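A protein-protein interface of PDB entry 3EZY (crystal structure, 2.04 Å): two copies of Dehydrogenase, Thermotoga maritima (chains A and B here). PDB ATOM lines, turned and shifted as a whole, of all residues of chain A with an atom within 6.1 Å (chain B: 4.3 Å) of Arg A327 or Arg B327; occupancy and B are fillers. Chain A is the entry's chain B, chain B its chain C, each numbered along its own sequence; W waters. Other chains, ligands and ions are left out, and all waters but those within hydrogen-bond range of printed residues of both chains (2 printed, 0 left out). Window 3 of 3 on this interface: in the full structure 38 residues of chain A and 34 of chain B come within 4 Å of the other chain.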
ATOM      1  N   VAL A 192     -23.202  21.758   4.827  1.00  0.00           N
ATOM      2  CA  VAL A 192     -24.086  22.656   5.563  1.00  0.00           C
ATOM      3  C   VAL A 192     -24.645  23.760   4.632  1.00  0.00           C
ATOM      4  O   VAL A 192     -23.931  24.250   3.731  1.00  0.00           O
ATOM      5  CB  VAL A 192     -23.278  23.342   6.727  1.00  0.00           C
ATOM      6  CG1 VAL A 192     -24.057  24.458   7.326  1.00  0.00           C
ATOM      7  CG2 VAL A 192     -22.881  22.322   7.792  1.00  0.00           C
ATOM      8  N   PHE A 193     -25.911  24.141   4.823  1.00  0.00           N
ATOM      9  CA  PHE A 193     -26.449  25.347   4.201  1.00  0.00           C
ATOM     10  C   PHE A 193     -27.010  26.187   5.319  1.00  0.00           C
ATOM     11  O   PHE A 193     -27.690  25.657   6.210  1.00  0.00           O
ATOM     12  CB  PHE A 193     -27.569  25.061   3.179  1.00  0.00           C
ATOM     13  CG  PHE A 193     -28.290  26.316   2.729  1.00  0.00           C
ATOM     14  CD1 PHE A 193     -27.782  27.093   1.674  1.00  0.00           C
ATOM     15  CD2 PHE A 193     -29.427  26.768   3.405  1.00  0.00           C
ATOM     16  CE1 PHE A 193     -28.422  28.265   1.282  1.00  0.00           C
ATOM     17  CE2 PHE A 193     -30.088  27.938   3.007  1.00  0.00           C
ATOM     18  CZ  PHE A 193     -29.569  28.698   1.940  1.00  0.00           C
ATOM     19  N   ALA A 194     -26.758  27.482   5.299  1.00  0.00           N
ATOM     20  CA  ALA A 194     -27.271  28.333   6.363  1.00  0.00           C
ATOM     21  C   ALA A 194     -27.866  29.609   5.832  1.00  0.00           C
ATOM     22  O   ALA A 194     -27.383  30.167   4.832  1.00  0.00           O
ATOM     23  CB  ALA A 194     -26.147  28.666   7.352  1.00  0.00           C
ATOM     24  N   ALA A 318     -18.243  26.798   8.353  1.00  0.00           N
ATOM     25  CA  ALA A 318     -18.949  26.405   7.132  1.00  0.00           C
ATOM     26  C   ALA A 318     -20.279  27.144   6.986  1.00  0.00           C
ATOM     27  O   ALA A 318     -20.675  27.532   5.881  1.00  0.00           O
ATOM     28  CB  ALA A 318     -19.197  24.896   7.115  1.00  0.00           C
ATOM     29  N   LYS A 321     -19.680  30.846   6.086  1.00  0.00           N
ATOM     30  CA  LYS A 321     -19.406  30.899   4.645  1.00  0.00           C
ATOM     31  C   LYS A 321     -20.675  30.702   3.800  1.00  0.00           C
ATOM     32  O   LYS A 321     -20.894  31.385   2.780  1.00  0.00           O
ATOM     33  CB  LYS A 321     -18.408  29.798   4.294  1.00  0.00           C
ATOM     34  CG  LYS A 321     -17.881  29.824   2.850  1.00  0.00           C
ATOM     35  CD  LYS A 321     -16.754  28.793   2.686  1.00  0.00           C
ATOM     36  CE  LYS A 321     -15.773  29.207   1.603  1.00  0.00           C
ATOM     37  NZ  LYS A 321     -15.127  28.009   0.949  1.00  0.00           N
ATOM     38  N   SER A 322     -21.515  29.747   4.203  1.00  0.00           N
ATOM     39  CA  SER A 322     -22.757  29.489   3.463  1.00  0.00           C
ATOM     40  C   SER A 322     -23.701  30.701   3.505  1.00  0.00           C
ATOM     41  O   SER A 322     -24.357  31.023   2.499  1.00  0.00           O
ATOM     42  CB  SER A 322     -23.452  28.234   3.992  1.00  0.00           C
ATOM     43  OG  SER A 322     -24.740  28.123   3.451  1.00  0.00           O
ATOM     44  N   LEU A 323     -23.773  31.376   4.651  1.00  0.00           N
ATOM     45  CA  LEU A 323     -24.669  32.508   4.755  1.00  0.00           C
ATOM     46  C   LEU A 323     -24.216  33.507   3.680  1.00  0.00           C
ATOM     47  O   LEU A 323     -25.001  33.934   2.801  1.00  0.00           O
ATOM     48  CB  LEU A 323     -24.639  33.113   6.167  1.00  0.00           C
ATOM     49  CG  LEU A 323     -25.388  34.430   6.402  1.00  0.00           C
ATOM     50  CD1 LEU A 323     -26.881  34.210   6.266  1.00  0.00           C
ATOM     51  CD2 LEU A 323     -25.094  35.058   7.753  1.00  0.00           C
ATOM     52  N   GLU A 324     -22.927  33.823   3.719  1.00  0.00           N
ATOM     53  CA  GLU A 324     -22.367  34.804   2.802  1.00  0.00           C
ATOM     54  C   GLU A 324     -22.429  34.380   1.325  1.00  0.00           C
ATOM     55  O   GLU A 324     -22.696  35.221   0.481  1.00  0.00           O
ATOM     56  CB  GLU A 324     -20.938  35.219   3.239  1.00  0.00           C
ATOM     57  CG  GLU A 324     -19.869  34.168   2.946  1.00  0.00           C
ATOM     58  CD  GLU A 324     -18.413  34.672   3.187  1.00  0.00           C
ATOM     59  OE1 GLU A 324     -17.628  34.721   2.192  1.00  0.00           O
ATOM     60  OE2 GLU A 324     -18.070  35.009   4.363  1.00  0.00           O
ATOM     61  N   GLU A 325     -22.239  33.097   1.009  1.00  0.00           N
ATOM     62  CA  GLU A 325     -22.194  32.660  -0.413  1.00  0.00           C
ATOM     63  C   GLU A 325     -23.501  32.106  -1.016  1.00  0.00           C
ATOM     64  O   GLU A 325     -23.575  31.715  -2.206  1.00  0.00           O
ATOM     65  CB  GLU A 325     -21.038  31.679  -0.627  1.00  0.00           C
ATOM     66  CG  GLU A 325     -19.702  32.390  -0.805  1.00  0.00           C
ATOM     67  CD  GLU A 325     -18.519  31.444  -0.919  1.00  0.00           C
ATOM     68  OE1 GLU A 325     -18.575  30.437  -1.659  1.00  0.00           O
ATOM     69  OE2 GLU A 325     -17.507  31.716  -0.254  1.00  0.00           O
ATOM     70  N   LYS A 326     -24.522  32.074  -0.167  1.00  0.00           N
ATOM     71  CA  LYS A 326     -25.853  31.600  -0.531  1.00  0.00           C
ATOM     72  C   LYS A 326     -25.831  30.221  -1.144  1.00  0.00           C
ATOM     73  O   LYS A 326     -26.567  29.928  -2.069  1.00  0.00           O
ATOM     74  CB  LYS A 326     -26.550  32.594  -1.455  1.00  0.00           C
ATOM     75  CG  LYS A 326     -26.600  33.996  -0.884  1.00  0.00           C
ATOM     76  CD  LYS A 326     -28.026  34.417  -0.593  1.00  0.00           C
ATOM     77  CE  LYS A 326     -28.606  33.748   0.692  1.00  0.00           C
ATOM     78  NZ  LYS A 326     -29.132  32.338   0.582  1.00  0.00           N
ATOM     79  N   ARG A 327     -25.023  29.341  -0.586  1.00  0.00           N
ATOM     80  CA  ARG A 327     -24.968  28.015  -1.126  1.00  0.00           C
ATOM     81  C   ARG A 327     -24.478  27.040  -0.065  1.00  0.00           C
ATOM     82  O   ARG A 327     -23.968  27.431   0.983  1.00  0.00           O
ATOM     83  CB  ARG A 327     -23.988  27.968  -2.294  1.00  0.00           C
ATOM     84  CG  ARG A 327     -22.580  28.243  -1.813  1.00  0.00           C
ATOM     85  CD  ARG A 327     -21.532  27.955  -2.900  1.00  0.00           C
ATOM     86  NE  ARG A 327     -20.222  28.336  -2.386  1.00  0.00           N
ATOM     87  CZ  ARG A 327     -19.337  27.494  -1.853  1.00  0.00           C
ATOM     88  NH1 ARG A 327     -18.165  27.942  -1.430  1.00  0.00           N
ATOM     89  NH2 ARG A 327     -19.599  26.206  -1.779  1.00  0.00           N
ATOM     90  N   SER A 328     -24.624  25.769  -0.380  1.00  0.00           N
ATOM     91  CA  SER A 328     -24.132  24.693   0.444  1.00  0.00           C
ATOM     92  C   SER A 328     -22.594  24.688   0.478  1.00  0.00           C
ATOM     93  O   SER A 328     -21.940  24.938  -0.554  1.00  0.00           O
ATOM     94  CB  SER A 328     -24.664  23.397  -0.154  1.00  0.00           C
ATOM     95  OG  SER A 328     -24.142  22.282   0.513  1.00  0.00           O
ATOM     96  N   VAL A 329     -22.014  24.376   1.642  1.00  0.00           N
ATOM     97  CA  VAL A 329     -20.557  24.409   1.836  1.00  0.00           C
ATOM     98  C   VAL A 329     -20.120  23.089   2.432  1.00  0.00           C
ATOM     99  O   VAL A 329     -20.630  22.663   3.482  1.00  0.00           O
ATOM    100  CB  VAL A 329     -20.111  25.605   2.732  1.00  0.00           C
ATOM    101  CG1 VAL A 329     -18.630  25.516   3.138  1.00  0.00           C
ATOM    102  CG2 VAL A 329     -20.345  26.905   2.014  1.00  0.00           C
ATOM    103  N   LYS A 330     -19.197  22.425   1.746  1.00  0.00           N
ATOM    104  CA  LYS A 330     -18.556  21.228   2.257  1.00  0.00           C
ATOM    105  C   LYS A 330     -17.579  21.518   3.369  1.00  0.00           C
ATOM    106  O   LYS A 330     -16.857  22.521   3.371  1.00  0.00           O
ATOM    107  CB  LYS A 330     -17.841  20.481   1.147  1.00  0.00           C
ATOM    108  CG  LYS A 330     -18.767  19.805   0.160  1.00  0.00           C
ATOM    109  CD  LYS A 330     -17.958  19.320  -1.016  1.00  0.00           C
ATOM    110  CE  LYS A 330     -18.842  18.715  -2.053  1.00  0.00           C
ATOM    111  NZ  LYS A 330     -19.049  17.273  -1.752  1.00  0.00           N
ATOM    112  N   GLU A 333     -14.086  22.300   2.596  1.00  0.00           N
ATOM    113  CA  GLU A 333     -13.752  23.657   2.206  1.00  0.00           C
ATOM    114  C   GLU A 333     -13.166  24.435   3.345  1.00  0.00           C
ATOM    115  O   GLU A 333     -12.491  25.427   3.135  1.00  0.00           O
ATOM    116  CB  GLU A 333     -14.980  24.421   1.731  1.00  0.00           C
ATOM    117  CG  GLU A 333     -15.722  23.799   0.603  1.00  0.00           C
ATOM    118  CD  GLU A 333     -16.716  24.772   0.026  1.00  0.00           C
ATOM    119  OE1 GLU A 333     -17.791  24.320  -0.454  1.00  0.00           O
ATOM    120  OE2 GLU A 333     -16.406  25.991   0.079  1.00  0.00           O
ATOM    121  N   PHE B 193     -33.983  26.975  -0.818  1.00  0.00           N
ATOM    122  CA  PHE B 193     -32.893  25.972  -0.894  1.00  0.00           C
ATOM    123  C   PHE B 193     -33.476  24.578  -0.602  1.00  0.00           C
ATOM    124  O   PHE B 193     -34.288  24.430   0.323  1.00  0.00           O
ATOM    125  CB  PHE B 193     -31.763  26.270   0.121  1.00  0.00           C
ATOM    126  CG  PHE B 193     -30.734  25.144   0.207  1.00  0.00           C
ATOM    127  CD1 PHE B 193     -29.696  25.065  -0.721  1.00  0.00           C
ATOM    128  CD2 PHE B 193     -30.851  24.142   1.175  1.00  0.00           C
ATOM    129  CE1 PHE B 193     -28.772  24.029  -0.684  1.00  0.00           C
ATOM    130  CE2 PHE B 193     -29.953  23.089   1.213  1.00  0.00           C
ATOM    131  CZ  PHE B 193     -28.895  23.039   0.284  1.00  0.00           C
ATOM    132  N   LYS B 321     -34.254  22.961  -8.955  1.00  0.00           N
ATOM    133  CA  LYS B 321     -33.023  23.606  -9.399  1.00  0.00           C
ATOM    134  C   LYS B 321     -31.993  23.743  -8.254  1.00  0.00           C
ATOM    135  O   LYS B 321     -30.792  23.553  -8.454  1.00  0.00           O
ATOM    136  CB  LYS B 321     -33.338  24.984  -9.989  1.00  0.00           C
ATOM    137  CG  LYS B 321     -32.147  25.601 -10.744  1.00  0.00           C
ATOM    138  CD  LYS B 321     -32.232  27.140 -10.744  1.00  0.00           C
ATOM    139  CE  LYS B 321     -31.940  27.749 -12.113  1.00  0.00           C
ATOM    140  NZ  LYS B 321     -30.729  27.143 -12.784  1.00  0.00           N
ATOM    141  N   SER B 322     -32.473  24.056  -7.046  1.00  0.00           N
ATOM    142  CA  SER B 322     -31.603  24.191  -5.869  1.00  0.00           C
ATOM    143  C   SER B 322     -30.945  22.867  -5.555  1.00  0.00           C
ATOM    144  O   SER B 322     -29.755  22.795  -5.248  1.00  0.00           O
ATOM    145  CB  SER B 322     -32.421  24.648  -4.648  1.00  0.00           C
ATOM    146  OG  SER B 322     -31.618  24.612  -3.474  1.00  0.00           O
ATOM    147  N   GLU B 325     -28.240  22.276  -8.314  1.00  0.00           N
ATOM    148  CA  GLU B 325     -27.164  23.249  -8.303  1.00  0.00           C
ATOM    149  C   GLU B 325     -26.507  23.522  -6.910  1.00  0.00           C
ATOM    150  O   GLU B 325     -25.473  24.222  -6.820  1.00  0.00           O
ATOM    151  CB  GLU B 325     -27.609  24.551  -9.011  1.00  0.00           C
ATOM    152  CG  GLU B 325     -27.575  24.430 -10.567  1.00  0.00           C
ATOM    153  CD  GLU B 325     -27.982  25.700 -11.343  1.00  0.00           C
ATOM    154  OE1 GLU B 325     -28.228  26.781 -10.743  1.00  0.00           O
ATOM    155  OE2 GLU B 325     -28.052  25.610 -12.593  1.00  0.00           O
ATOM    156  N   LYS B 326     -27.106  22.983  -5.836  1.00  0.00           N
ATOM    157  CA  LYS B 326     -26.552  23.082  -4.495  1.00  0.00           C
ATOM    158  C   LYS B 326     -26.387  24.499  -3.998  1.00  0.00           C
ATOM    159  O   LYS B 326     -25.420  24.821  -3.317  1.00  0.00           O
ATOM    160  CB  LYS B 326     -25.219  22.358  -4.443  1.00  0.00           C
ATOM    161  CG  LYS B 326     -25.261  20.997  -5.145  1.00  0.00           C
ATOM    162  CD  LYS B 326     -25.399  19.909  -4.150  1.00  0.00           C
ATOM    163  CE  LYS B 326     -24.387  18.794  -4.434  1.00  0.00           C
ATOM    164  NZ  LYS B 326     -24.039  18.005  -3.193  1.00  0.00           N
ATOM    165  N   ARG B 327     -27.339  25.352  -4.329  1.00  0.00           N
ATOM    166  CA  ARG B 327     -27.344  26.684  -3.817  1.00  0.00           C
ATOM    167  C   ARG B 327     -28.791  27.157  -3.688  1.00  0.00           C
ATOM    168  O   ARG B 327     -29.721  26.535  -4.211  1.00  0.00           O
ATOM    169  CB  ARG B 327     -26.606  27.617  -4.796  1.00  0.00           C
ATOM    170  CG  ARG B 327     -27.332  27.729  -6.150  1.00  0.00           C
ATOM    171  CD  ARG B 327     -26.588  28.651  -7.095  1.00  0.00           C
ATOM    172  NE  ARG B 327     -27.123  28.574  -8.447  1.00  0.00           N
ATOM    173  CZ  ARG B 327     -28.116  29.323  -8.884  1.00  0.00           C
ATOM    174  NH1 ARG B 327     -28.521  29.204 -10.133  1.00  0.00           N
ATOM    175  NH2 ARG B 327     -28.680  30.207  -8.070  1.00  0.00           N
ATOM    176  N   SER B 328     -28.955  28.301  -3.058  1.00  0.00           N
ATOM    177  CA  SER B 328     -30.242  28.958  -2.933  1.00  0.00           C
ATOM    178  C   SER B 328     -30.682  29.523  -4.309  1.00  0.00           C
ATOM    179  O   SER B 328     -29.868  30.100  -5.039  1.00  0.00           O
ATOM    180  CB  SER B 328     -30.070  30.061  -1.890  1.00  0.00           C
ATOM    181  OG  SER B 328     -31.254  30.775  -1.715  1.00  0.00           O
ATOM    182  N   VAL B 329     -31.950  29.346  -4.674  1.00  0.00           N
ATOM    183  CA  VAL B 329     -32.452  29.783  -5.973  1.00  0.00           C
ATOM    184  C   VAL B 329     -33.583  30.781  -5.833  1.00  0.00           C
ATOM    185  O   VAL B 329     -34.608  30.477  -5.215  1.00  0.00           O
ATOM    186  CB  VAL B 329     -32.996  28.585  -6.755  1.00  0.00           C
ATOM    187  CG1 VAL B 329     -33.831  29.053  -7.960  1.00  0.00           C
ATOM    188  CG2 VAL B 329     -31.843  27.642  -7.165  1.00  0.00           C
ATOM    189  N   GLU B 333     -35.399  33.381 -11.112  1.00  0.00           N
ATOM    190  CA  GLU B 333     -34.665  32.507 -12.026  1.00  0.00           C
ATOM    191  C   GLU B 333     -35.542  31.457 -12.653  1.00  0.00           C
ATOM    192  O   GLU B 333     -35.164  30.830 -13.635  1.00  0.00           O
ATOM    193  CB  GLU B 333     -33.550  31.760 -11.290  1.00  0.00           C
ATOM    194  CG  GLU B 333     -32.606  32.636 -10.478  1.00  0.00           C
ATOM    195  CD  GLU B 333     -31.599  31.814  -9.689  1.00  0.00           C
ATOM    196  OE1 GLU B 333     -31.022  30.871 -10.286  1.00  0.00           O
ATOM    197  OE2 GLU B 333     -31.386  32.119  -8.483  1.00  0.00           O
HETATM  198  O   HOH W   1     -27.485  31.599  -4.807  1.00  0.00           O
HETATM  199  O   HOH W   2     -22.506  24.756  -3.217  1.00  0.00           O
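The backbone carbonyl oxygen (O) of Lys A326 is in hydrogen-bond range of the backbone NH (N) of Ser B328 (3.1 Å). O of Lys B326 sits at hydrogen-bond distance from N of Ser A328 (3.2 Å).
The side-chain carboxylate of Glu B325 lies within salt-bridge range of the guanidinium group of Arg B327. The side-chain carboxylate (OE1) of Glu B333 is in salt-bridge range of the guanidinium group (NH1) of Arg B327, 3.0 Å away. The backbone carbonyl oxygen (O) of Arg A327 lies within hydrogen-bond range of the side-chain hydroxyl (OG) of Ser A322, at 2.7 Å. O of Arg B327 lies within hydrogen-bond range of OG of Ser B322 (2.8 Å). The side-chain carboxylate (OE1) of Glu A333 is in salt-bridge range of the guanidinium group (NH2) of Arg A327. The side-chain carboxylate (OE1) of Glu A325 is in salt-bridge range of the guanidinium group (NH1) of Arg A327 (2.5 Å).
CB of Phe A193 touches CE2 of Phe B193, at 3.7 Å. O of Lys A326 touches CB of Arg B327, at 3.6 Å. Arg A327 touches Lys B326. Arg A327 touches Arg B327 (CB to CB, 3.6 Å).
Of chain B, only Lys B326 (3.6 Å) and Arg B327 (3.6 Å) come within 4 Å of Arg A327. Of the printed residues of chain B, Ser A328 touches Lys B326 (3.2 Å). Of the printed residues of chain A, Lys B326 touches Arg A327 and Ser A328. Arg B327 touches just these residues of chain A: Lys A326 and Arg A327. The nearest residue of chain A that does not touch Arg B327 is Ser A328 (4.5 Å).
Of the 15 printed residues of chain A, 4 touch a printed residue of chain B. Printed residues of chain B that touch a printed residue of chain A: Phe B193, Lys B326, Arg B327 and Ser B328.
Phe A193 touches its own counterpart, Phe B193. Lys A326 touches Arg B327, and with the chains exchanged Arg A327 touches Lys B326. Lys A326 touches Ser B328, and with the chains exchanged Ser A328 touches Lys B326. Arg B327 touches its own counterpart, Arg A327. Positions printed for both chains: 193, 321, 322, 325, 326, 327, 328, 329 and 333.
Water W2 lies within hydrogen-bond range of O of Ser A328 and O of Lys B326. Water W1 bridges O of Ser B328 (2.8 Å) and O of Lys A326 (3.3 Å).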
